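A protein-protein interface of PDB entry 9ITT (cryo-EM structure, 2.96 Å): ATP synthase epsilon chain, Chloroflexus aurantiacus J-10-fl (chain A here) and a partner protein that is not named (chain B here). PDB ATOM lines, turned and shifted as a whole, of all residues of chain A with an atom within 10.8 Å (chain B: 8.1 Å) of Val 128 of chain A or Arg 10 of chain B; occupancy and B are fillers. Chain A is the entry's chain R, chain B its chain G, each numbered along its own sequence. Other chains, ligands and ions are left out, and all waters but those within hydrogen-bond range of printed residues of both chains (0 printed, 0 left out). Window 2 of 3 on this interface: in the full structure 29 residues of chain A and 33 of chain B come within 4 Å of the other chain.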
ATOM      1  N   ARG A 120      31.136  -9.581 -22.867  1.00  0.00           N
ATOM      2  CA  ARG A 120      30.923 -10.789 -22.078  1.00  0.00           C
ATOM      3  C   ARG A 120      30.306 -11.881 -22.922  1.00  0.00           C
ATOM      4  O   ARG A 120      30.709 -13.046 -22.809  1.00  0.00           O
ATOM      5  CB  ARG A 120      30.037 -10.502 -20.867  1.00  0.00           C
ATOM      6  CG  ARG A 120      30.749  -9.809 -19.714  1.00  0.00           C
ATOM      7  CD  ARG A 120      30.002 -10.017 -18.404  1.00  0.00           C
ATOM      8  NE  ARG A 120      28.589  -9.689 -18.535  1.00  0.00           N
ATOM      9  CZ  ARG A 120      28.027  -8.532 -18.199  1.00  0.00           C
ATOM     10  NH1 ARG A 120      28.728  -7.540 -17.672  1.00  0.00           N
ATOM     11  NH2 ARG A 120      26.723  -8.362 -18.402  1.00  0.00           N
ATOM     12  N   LYS A 121      29.369 -11.510 -23.800  1.00  0.00           N
ATOM     13  CA  LYS A 121      28.948 -12.417 -24.853  1.00  0.00           C
ATOM     14  C   LYS A 121      30.167 -12.991 -25.560  1.00  0.00           C
ATOM     15  O   LYS A 121      30.541 -14.125 -25.288  1.00  0.00           O
ATOM     16  CB  LYS A 121      28.025 -11.689 -25.829  1.00  0.00           C
ATOM     17  CG  LYS A 121      27.325 -12.592 -26.819  1.00  0.00           C
ATOM     18  CD  LYS A 121      26.444 -11.791 -27.751  1.00  0.00           C
ATOM     19  CE  LYS A 121      25.157 -11.360 -27.074  1.00  0.00           C
ATOM     20  NZ  LYS A 121      24.231 -10.682 -28.021  1.00  0.00           N
ATOM     21  N   GLU A 122      30.922 -12.151 -26.280  1.00  0.00           N
ATOM     22  CA  GLU A 122      32.001 -12.647 -27.144  1.00  0.00           C
ATOM     23  C   GLU A 122      32.921 -13.619 -26.405  1.00  0.00           C
ATOM     24  O   GLU A 122      33.191 -14.738 -26.876  1.00  0.00           O
ATOM     25  CB  GLU A 122      32.816 -11.467 -27.673  1.00  0.00           C
ATOM     26  CG  GLU A 122      32.090 -10.587 -28.665  1.00  0.00           C
ATOM     27  CD  GLU A 122      32.890  -9.355 -29.041  1.00  0.00           C
ATOM     28  OE1 GLU A 122      34.083  -9.288 -28.679  1.00  0.00           O
ATOM     29  OE2 GLU A 122      32.329  -8.454 -29.699  1.00  0.00           O
ATOM     30  N   MET A 123      33.365 -13.220 -25.213  1.00  0.00           N
ATOM     31  CA  MET A 123      34.282 -14.053 -24.442  1.00  0.00           C
ATOM     32  C   MET A 123      33.649 -15.388 -24.065  1.00  0.00           C
ATOM     33  O   MET A 123      34.227 -16.448 -24.323  1.00  0.00           O
ATOM     34  CB  MET A 123      34.755 -13.327 -23.183  1.00  0.00           C
ATOM     35  CG  MET A 123      35.999 -12.480 -23.384  1.00  0.00           C
ATOM     36  SD  MET A 123      36.868 -12.254 -21.831  1.00  0.00           S
ATOM     37  CE  MET A 123      38.377 -11.459 -22.389  1.00  0.00           C
ATOM     38  N   VAL A 124      32.461 -15.366 -23.449  1.00  0.00           N
ATOM     39  CA  VAL A 124      31.866 -16.620 -22.989  1.00  0.00           C
ATOM     40  C   VAL A 124      31.284 -17.433 -24.135  1.00  0.00           C
ATOM     41  O   VAL A 124      31.018 -18.630 -23.963  1.00  0.00           O
ATOM     42  CB  VAL A 124      30.826 -16.305 -21.893  1.00  0.00           C
ATOM     43  CG1 VAL A 124      29.554 -15.732 -22.493  1.00  0.00           C
ATOM     44  CG2 VAL A 124      30.534 -17.536 -21.039  1.00  0.00           C
ATOM     45  N   ARG A 125      31.080 -16.816 -25.300  1.00  0.00           N
ATOM     46  CA  ARG A 125      30.765 -17.527 -26.531  1.00  0.00           C
ATOM     47  C   ARG A 125      31.942 -18.362 -26.999  1.00  0.00           C
ATOM     48  O   ARG A 125      31.771 -19.536 -27.345  1.00  0.00           O
ATOM     49  CB  ARG A 125      30.370 -16.528 -27.624  1.00  0.00           C
ATOM     50  CG  ARG A 125      29.108 -15.731 -27.330  1.00  0.00           C
ATOM     51  CD  ARG A 125      27.882 -16.546 -27.526  1.00  0.00           C
ATOM     52  NE  ARG A 125      27.701 -16.876 -28.930  1.00  0.00           N
ATOM     53  CZ  ARG A 125      27.262 -18.035 -29.399  1.00  0.00           C
ATOM     54  NH1 ARG A 125      27.052 -19.079 -28.611  1.00  0.00           N
ATOM     55  NH2 ARG A 125      27.029 -18.152 -30.699  1.00  0.00           N
ATOM     56  N   LEU A 126      33.139 -17.782 -27.017  1.00  0.00           N
ATOM     57  CA  LEU A 126      34.316 -18.550 -27.414  1.00  0.00           C
ATOM     58  C   LEU A 126      34.929 -19.352 -26.278  1.00  0.00           C
ATOM     59  O   LEU A 126      35.896 -20.084 -26.514  1.00  0.00           O
ATOM     60  CB  LEU A 126      35.367 -17.639 -28.036  1.00  0.00           C
ATOM     61  CG  LEU A 126      35.078 -17.529 -29.530  1.00  0.00           C
ATOM     62  CD1 LEU A 126      35.654 -16.282 -30.082  1.00  0.00           C
ATOM     63  CD2 LEU A 126      35.618 -18.749 -30.292  1.00  0.00           C
ATOM     64  N   ARG A 127      34.400 -19.243 -25.064  1.00  0.00           N
ATOM     65  CA  ARG A 127      34.686 -20.256 -24.058  1.00  0.00           C
ATOM     66  C   ARG A 127      33.940 -21.553 -24.334  1.00  0.00           C
ATOM     67  O   ARG A 127      34.333 -22.600 -23.812  1.00  0.00           O
ATOM     68  CB  ARG A 127      34.333 -19.737 -22.664  1.00  0.00           C
ATOM     69  CG  ARG A 127      35.370 -18.781 -22.092  1.00  0.00           C
ATOM     70  CD  ARG A 127      35.084 -18.416 -20.644  1.00  0.00           C
ATOM     71  NE  ARG A 127      35.163 -19.568 -19.753  1.00  0.00           N
ATOM     72  CZ  ARG A 127      35.283 -19.498 -18.433  1.00  0.00           C
ATOM     73  NH1 ARG A 127      35.343 -18.335 -17.801  1.00  0.00           N
ATOM     74  NH2 ARG A 127      35.347 -20.623 -17.727  1.00  0.00           N
ATOM     75  N   VAL A 128      32.886 -21.509 -25.153  1.00  0.00           N
ATOM     76  CA  VAL A 128      32.195 -22.733 -25.545  1.00  0.00           C
ATOM     77  C   VAL A 128      33.119 -23.620 -26.369  1.00  0.00           C
ATOM     78  O   VAL A 128      33.134 -24.846 -26.206  1.00  0.00           O
ATOM     79  CB  VAL A 128      30.903 -22.395 -26.312  1.00  0.00           C
ATOM     80  CG1 VAL A 128      30.158 -23.669 -26.685  1.00  0.00           C
ATOM     81  CG2 VAL A 128      30.015 -21.471 -25.488  1.00  0.00           C
ATOM     82  N   ALA A 129      33.896 -23.022 -27.265  1.00  0.00           N
ATOM     83  CA  ALA A 129      34.822 -23.773 -28.105  1.00  0.00           C
ATOM     84  C   ALA A 129      35.858 -24.500 -27.254  1.00  0.00           C
ATOM     85  O   ALA A 129      35.783 -25.716 -27.077  1.00  0.00           O
ATOM     86  CB  ALA A 129      35.507 -22.844 -29.095  1.00  0.00           C
ATOM     87  N   PRO B   2      34.130 -33.501 -23.473  1.00  0.00           N
ATOM     88  CA  PRO B   2      33.029 -34.382 -23.075  1.00  0.00           C
ATOM     89  C   PRO B   2      33.421 -35.348 -21.958  1.00  0.00           C
ATOM     90  O   PRO B   2      33.530 -36.555 -22.178  1.00  0.00           O
ATOM     91  CB  PRO B   2      32.699 -35.123 -24.375  1.00  0.00           C
ATOM     92  CG  PRO B   2      33.042 -34.149 -25.437  1.00  0.00           C
ATOM     93  CD  PRO B   2      34.258 -33.416 -24.937  1.00  0.00           C
ATOM     94  N   ARG B   5      32.603 -32.638 -17.031  1.00  0.00           N
ATOM     95  CA  ARG B   5      33.100 -31.429 -16.388  1.00  0.00           C
ATOM     96  C   ARG B   5      33.362 -30.327 -17.398  1.00  0.00           C
ATOM     97  O   ARG B   5      33.134 -29.155 -17.096  1.00  0.00           O
ATOM     98  CB  ARG B   5      34.384 -31.736 -15.605  1.00  0.00           C
ATOM     99  CG  ARG B   5      34.842 -30.606 -14.699  1.00  0.00           C
ATOM    100  CD  ARG B   5      36.055 -31.005 -13.878  1.00  0.00           C
ATOM    101  NE  ARG B   5      37.186 -31.393 -14.716  1.00  0.00           N
ATOM    102  CZ  ARG B   5      38.100 -30.561 -15.199  1.00  0.00           C
ATOM    103  NH1 ARG B   5      38.050 -29.259 -14.966  1.00  0.00           N
ATOM    104  NH2 ARG B   5      39.091 -31.048 -15.938  1.00  0.00           N
ATOM    105  N   GLU B   6      33.847 -30.678 -18.589  1.00  0.00           N
ATOM    106  CA  GLU B   6      33.882 -29.720 -19.683  1.00  0.00           C
ATOM    107  C   GLU B   6      32.477 -29.356 -20.136  1.00  0.00           C
ATOM    108  O   GLU B   6      32.211 -28.193 -20.461  1.00  0.00           O
ATOM    109  CB  GLU B   6      34.681 -30.293 -20.851  1.00  0.00           C
ATOM    110  CG  GLU B   6      36.134 -30.595 -20.522  1.00  0.00           C
ATOM    111  CD  GLU B   6      36.864 -31.254 -21.675  1.00  0.00           C
ATOM    112  OE1 GLU B   6      36.208 -31.581 -22.685  1.00  0.00           O
ATOM    113  OE2 GLU B   6      38.094 -31.445 -21.571  1.00  0.00           O
ATOM    114  N   ILE B   7      31.566 -30.332 -20.162  1.00  0.00           N
ATOM    115  CA  ILE B   7      30.194 -30.040 -20.560  1.00  0.00           C
ATOM    116  C   ILE B   7      29.528 -29.154 -19.520  1.00  0.00           C
ATOM    117  O   ILE B   7      28.690 -28.315 -19.860  1.00  0.00           O
ATOM    118  CB  ILE B   7      29.380 -31.329 -20.789  1.00  0.00           C
ATOM    119  CG1 ILE B   7      30.083 -32.277 -21.767  1.00  0.00           C
ATOM    120  CG2 ILE B   7      28.012 -30.984 -21.369  1.00  0.00           C
ATOM    121  CD1 ILE B   7      29.502 -33.677 -21.776  1.00  0.00           C
ATOM    122  N   LYS B   8      29.859 -29.333 -18.241  1.00  0.00           N
ATOM    123  CA  LYS B   8      29.305 -28.460 -17.212  1.00  0.00           C
ATOM    124  C   LYS B   8      29.752 -27.019 -17.429  1.00  0.00           C
ATOM    125  O   LYS B   8      28.949 -26.083 -17.316  1.00  0.00           O
ATOM    126  CB  LYS B   8      29.730 -28.961 -15.833  1.00  0.00           C
ATOM    127  CG  LYS B   8      29.148 -28.200 -14.652  1.00  0.00           C
ATOM    128  CD  LYS B   8      27.645 -28.383 -14.550  1.00  0.00           C
ATOM    129  CE  LYS B   8      27.094 -27.699 -13.312  1.00  0.00           C
ATOM    130  NZ  LYS B   8      25.610 -27.790 -13.235  1.00  0.00           N
ATOM    131  N   ARG B   9      31.031 -26.827 -17.751  1.00  0.00           N
ATOM    132  CA  ARG B   9      31.531 -25.493 -18.060  1.00  0.00           C
ATOM    133  C   ARG B   9      30.842 -24.923 -19.291  1.00  0.00           C
ATOM    134  O   ARG B   9      30.500 -23.735 -19.327  1.00  0.00           O
ATOM    135  CB  ARG B   9      33.042 -25.553 -18.264  1.00  0.00           C
ATOM    136  CG  ARG B   9      33.737 -24.195 -18.246  1.00  0.00           C
ATOM    137  CD  ARG B   9      35.176 -24.247 -18.767  1.00  0.00           C
ATOM    138  NE  ARG B   9      35.323 -25.042 -19.983  1.00  0.00           N
ATOM    139  CZ  ARG B   9      35.132 -24.589 -21.214  1.00  0.00           C
ATOM    140  NH1 ARG B   9      34.758 -23.341 -21.447  1.00  0.00           N
ATOM    141  NH2 ARG B   9      35.309 -25.414 -22.243  1.00  0.00           N
ATOM    142  N   ARG B  10      30.631 -25.754 -20.314  1.00  0.00           N
ATOM    143  CA  ARG B  10      29.913 -25.300 -21.500  1.00  0.00           C
ATOM    144  C   ARG B  10      28.496 -24.868 -21.151  1.00  0.00           C
ATOM    145  O   ARG B  10      28.003 -23.856 -21.661  1.00  0.00           O
ATOM    146  CB  ARG B  10      29.883 -26.410 -22.551  1.00  0.00           C
ATOM    147  CG  ARG B  10      31.033 -26.378 -23.552  1.00  0.00           C
ATOM    148  CD  ARG B  10      30.722 -27.201 -24.803  1.00  0.00           C
ATOM    149  NE  ARG B  10      31.534 -26.790 -25.945  1.00  0.00           N
ATOM    150  CZ  ARG B  10      31.140 -26.789 -27.215  1.00  0.00           C
ATOM    151  NH1 ARG B  10      29.935 -27.205 -27.575  1.00  0.00           N
ATOM    152  NH2 ARG B  10      31.982 -26.363 -28.152  1.00  0.00           N
ATOM    153  N   ILE B  11      27.819 -25.635 -20.298  1.00  0.00           N
ATOM    154  CA  ILE B  11      26.451 -25.301 -19.914  1.00  0.00           C
ATOM    155  C   ILE B  11      26.425 -23.972 -19.178  1.00  0.00           C
ATOM    156  O   ILE B  11      25.561 -23.123 -19.427  1.00  0.00           O
ATOM    157  CB  ILE B  11      25.847 -26.432 -19.063  1.00  0.00           C
ATOM    158  CG1 ILE B  11      25.583 -27.660 -19.932  1.00  0.00           C
ATOM    159  CG2 ILE B  11      24.556 -25.971 -18.401  1.00  0.00           C
ATOM    160  CD1 ILE B  11      25.402 -28.939 -19.151  1.00  0.00           C
ATOM    161  N   ARG B  12      27.373 -23.769 -18.261  1.00  0.00           N
ATOM    162  CA  ARG B  12      27.461 -22.488 -17.568  1.00  0.00           C
ATOM    163  C   ARG B  12      27.691 -21.351 -18.556  1.00  0.00           C
ATOM    164  O   ARG B  12      27.073 -20.283 -18.450  1.00  0.00           O
ATOM    165  CB  ARG B  12      28.588 -22.535 -16.538  1.00  0.00           C
ATOM    166  CG  ARG B  12      28.356 -21.676 -15.313  1.00  0.00           C
ATOM    167  CD  ARG B  12      29.659 -21.416 -14.569  1.00  0.00           C
ATOM    168  NE  ARG B  12      30.523 -22.592 -14.533  1.00  0.00           N
ATOM    169  CZ  ARG B  12      30.279 -23.692 -13.830  1.00  0.00           C
ATOM    170  NH1 ARG B  12      29.190 -23.816 -13.088  1.00  0.00           N
ATOM    171  NH2 ARG B  12      31.150 -24.695 -13.875  1.00  0.00           N
ATOM    172  N   SER B  13      28.571 -21.573 -19.532  1.00  0.00           N
ATOM    173  CA  SER B  13      28.865 -20.548 -20.525  1.00  0.00           C
ATOM    174  C   SER B  13      27.619 -20.169 -21.315  1.00  0.00           C
ATOM    175  O   SER B  13      27.302 -18.983 -21.463  1.00  0.00           O
ATOM    176  CB  SER B  13      29.965 -21.047 -21.461  1.00  0.00           C
ATOM    177  OG  SER B  13      30.119 -20.199 -22.583  1.00  0.00           O
ATOM    178  N   VAL B  14      26.893 -21.163 -21.827  1.00  0.00           N
ATOM    179  CA  VAL B  14      25.731 -20.841 -22.650  1.00  0.00           C
ATOM    180  C   VAL B  14      24.613 -20.260 -21.793  1.00  0.00           C
ATOM    181  O   VAL B  14      23.808 -19.462 -22.283  1.00  0.00           O
ATOM    182  CB  VAL B  14      25.253 -22.062 -23.455  1.00  0.00           C
ATOM    183  CG1 VAL B  14      24.151 -21.652 -24.418  1.00  0.00           C
ATOM    184  CG2 VAL B  14      26.394 -22.658 -24.257  1.00  0.00           C
ATOM    185  N   LYS B  15      24.529 -20.634 -20.516  1.00  0.00           N
ATOM    186  CA  LYS B  15      23.569 -19.973 -19.639  1.00  0.00           C
ATOM    187  C   LYS B  15      23.901 -18.495 -19.483  1.00  0.00           C
ATOM    188  O   LYS B  15      23.003 -17.644 -19.504  1.00  0.00           O
ATOM    189  CB  LYS B  15      23.532 -20.661 -18.277  1.00  0.00           C
ATOM    190  CG  LYS B  15      22.721 -21.941 -18.255  1.00  0.00           C
ATOM    191  CD  LYS B  15      22.680 -22.541 -16.862  1.00  0.00           C
ATOM    192  CE  LYS B  15      21.990 -23.891 -16.859  1.00  0.00           C
ATOM    193  NZ  LYS B  15      20.521 -23.758 -17.052  1.00  0.00           N
ATOM    194  N   ASN B  16      25.187 -18.170 -19.328  1.00  0.00           N
ATOM    195  CA  ASN B  16      25.582 -16.766 -19.287  1.00  0.00           C
ATOM    196  C   ASN B  16      25.222 -16.062 -20.589  1.00  0.00           C
ATOM    197  O   ASN B  16      24.762 -14.912 -20.579  1.00  0.00           O
ATOM    198  CB  ASN B  16      27.080 -16.649 -19.013  1.00  0.00           C
ATOM    199  CG  ASN B  16      27.441 -17.005 -17.588  1.00  0.00           C
ATOM    200  OD1 ASN B  16      26.569 -17.144 -16.730  1.00  0.00           O
ATOM    201  ND2 ASN B  16      28.733 -17.158 -17.326  1.00  0.00           N
ATOM    202  N   VAL B  17      25.430 -16.740 -21.720  1.00  0.00           N
ATOM    203  CA  VAL B  17      25.048 -16.172 -23.012  1.00  0.00           C
ATOM    204  C   VAL B  17      23.559 -15.859 -23.024  1.00  0.00           C
ATOM    205  O   VAL B  17      23.134 -14.791 -23.475  1.00  0.00           O
ATOM    206  CB  VAL B  17      25.411 -17.133 -24.157  1.00  0.00           C
ATOM    207  CG1 VAL B  17      24.799 -16.656 -25.468  1.00  0.00           C
ATOM    208  CG2 VAL B  17      26.899 -17.273 -24.290  1.00  0.00           C
ATOM    209  N   ALA B 255      20.263 -20.190 -27.556  1.00  0.00           N
ATOM    210  CA  ALA B 255      21.068 -20.512 -26.387  1.00  0.00           C
ATOM    211  C   ALA B 255      20.331 -21.452 -25.449  1.00  0.00           C
ATOM    212  O   ALA B 255      20.942 -22.358 -24.883  1.00  0.00           O
ATOM    213  CB  ALA B 255      21.463 -19.233 -25.650  1.00  0.00           C
ATOM    214  N   LEU B 258      20.511 -24.870 -27.023  1.00  0.00           N
ATOM    215  CA  LEU B 258      21.834 -25.448 -26.844  1.00  0.00           C
ATOM    216  C   LEU B 258      22.075 -25.849 -25.399  1.00  0.00           C
ATOM    217  O   LEU B 258      22.770 -26.834 -25.146  1.00  0.00           O
ATOM    218  CB  LEU B 258      22.910 -24.468 -27.308  1.00  0.00           C
ATOM    219  CG  LEU B 258      24.246 -25.113 -27.683  1.00  0.00           C
ATOM    220  CD1 LEU B 258      24.128 -25.905 -28.977  1.00  0.00           C
ATOM    221  CD2 LEU B 258      25.340 -24.074 -27.805  1.00  0.00           C
ATOM    222  N   VAL B 259      21.521 -25.108 -24.439  1.00  0.00           N
ATOM    223  CA  VAL B 259      21.622 -25.514 -23.040  1.00  0.00           C
ATOM    224  C   VAL B 259      20.898 -26.833 -22.828  1.00  0.00           C
ATOM    225  O   VAL B 259      21.376 -27.705 -22.102  1.00  0.00           O
ATOM    226  CB  VAL B 259      21.070 -24.416 -22.113  1.00  0.00           C
ATOM    227  CG1 VAL B 259      20.857 -24.956 -20.707  1.00  0.00           C
ATOM    228  CG2 VAL B 259      22.017 -23.249 -22.072  1.00  0.00           C
ATOM    229  N   LEU B 262      23.122 -29.545 -24.402  1.00  0.00           N
ATOM    230  CA  LEU B 262      24.310 -29.755 -23.588  1.00  0.00           C
ATOM    231  C   LEU B 262      23.964 -30.411 -22.262  1.00  0.00           C
ATOM    232  O   LEU B 262      24.764 -31.181 -21.735  1.00  0.00           O
ATOM    233  CB  LEU B 262      25.023 -28.427 -23.348  1.00  0.00           C
ATOM    234  CG  LEU B 262      25.889 -27.893 -24.489  1.00  0.00           C
ATOM    235  CD1 LEU B 262      26.266 -26.452 -24.218  1.00  0.00           C
ATOM    236  CD2 LEU B 262      27.134 -28.740 -24.674  1.00  0.00           C
ATOM    237  N   THR B 263      22.789 -30.118 -21.704  1.00  0.00           N
ATOM    238  CA  THR B 263      22.355 -30.805 -20.498  1.00  0.00           C
ATOM    239  C   THR B 263      22.119 -32.282 -20.769  1.00  0.00           C
ATOM    240  O   THR B 263      22.473 -33.132 -19.948  1.00  0.00           O
ATOM    241  CB  THR B 263      21.088 -30.156 -19.947  1.00  0.00           C
ATOM    242  OG1 THR B 263      21.319 -28.759 -19.724  1.00  0.00           O
ATOM    243  CG2 THR B 263      20.675 -30.807 -18.641  1.00  0.00           C
ATOM    244  N   SER B 265      23.669 -34.045 -23.062  1.00  0.00           N
ATOM    245  CA  SER B 265      25.004 -34.619 -23.200  1.00  0.00           C
ATOM    246  C   SER B 265      25.683 -34.772 -21.843  1.00  0.00           C
ATOM    247  O   SER B 265      26.355 -35.777 -21.587  1.00  0.00           O
ATOM    248  CB  SER B 265      25.851 -33.754 -24.129  1.00  0.00           C
ATOM    249  OG  SER B 265      27.090 -34.378 -24.409  1.00  0.00           O
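The backbone carbonyl oxygen (O) of Arg 127 of chain A lies within hydrogen-bond range of the guanidinium group (NH1) of Arg 9 of chain B (2.5 Å).
The guanidinium group of Arg 10 of chain B lies within hydrogen-bond range of the backbone carbonyl oxygen of Val 128 of chain A.
O of Val 124 of chain A lies close to OG of Ser 13 of chain B, at 2.3 Å.
Hydrophobic or aromatic side chains of chain B within 4 Å of the printed part of chain A: Val 17.
Printed residues of chain A that touch a printed residue of chain B: Val 124, Arg 125, Arg 127, Val 128 and Ala 129.
Among the printed residues, 7 pairs touch across the chains.
Among the printed residues, no Asp or Glu carboxylate lies within 4 Å of a Lys or Arg side-chain nitrogen of the other chain.
Among the printed residues, pairs that only touch across the chains: Val 124 of chain A with Val 17 of chain B, Arg 125 of chain A with Val 17 of chain B, Val 128 of chain A with Ser 13 of chain B and Ala 129 of chain A with Arg 10 of chain B.
Printed residues of chain B within 4 Å of Val 128 of chain A: Arg 10 (2.5 Å) and Ser 13 (3.2 Å).
Of chain A, only Val 128 and Ala 129 come within 4 Å of Arg 10 of chain B.
Ala 129 of chain A touches just one residue of chain B: Arg 10.
Arg 9 of chain B touches just one residue of chain A: Arg 127 (2.5 Å).
Ile 11 of chain B touches none of the printed residues of chain A.
Of chain A, only Val 124 (2.3 Å) and Val 128 (3.2 Å) come within 4 Å of Ser 13 of chain B.
Printed residues of chain B within 4 Å of Arg 127 of chain A: Arg 9 (2.5 Å).
Printed residues of chain B within 4 Å of Val 124 of chain A: Ser 13 (2.3 Å) and Val 17 (3.6 Å).
Printed residues of chain B within 4 Å of Arg 125 of chain A: Val 17 (3.5 Å).
Printed residues of chain A within 4 Å of Val 17 of chain B: Val 124 and Arg 125.
Glu 6 of chain B touches none of the printed residues of chain A.
The nearest printed residue of chain B that does not touch Val 128 of chain A is Val 14 of chain B (4.004 Å).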
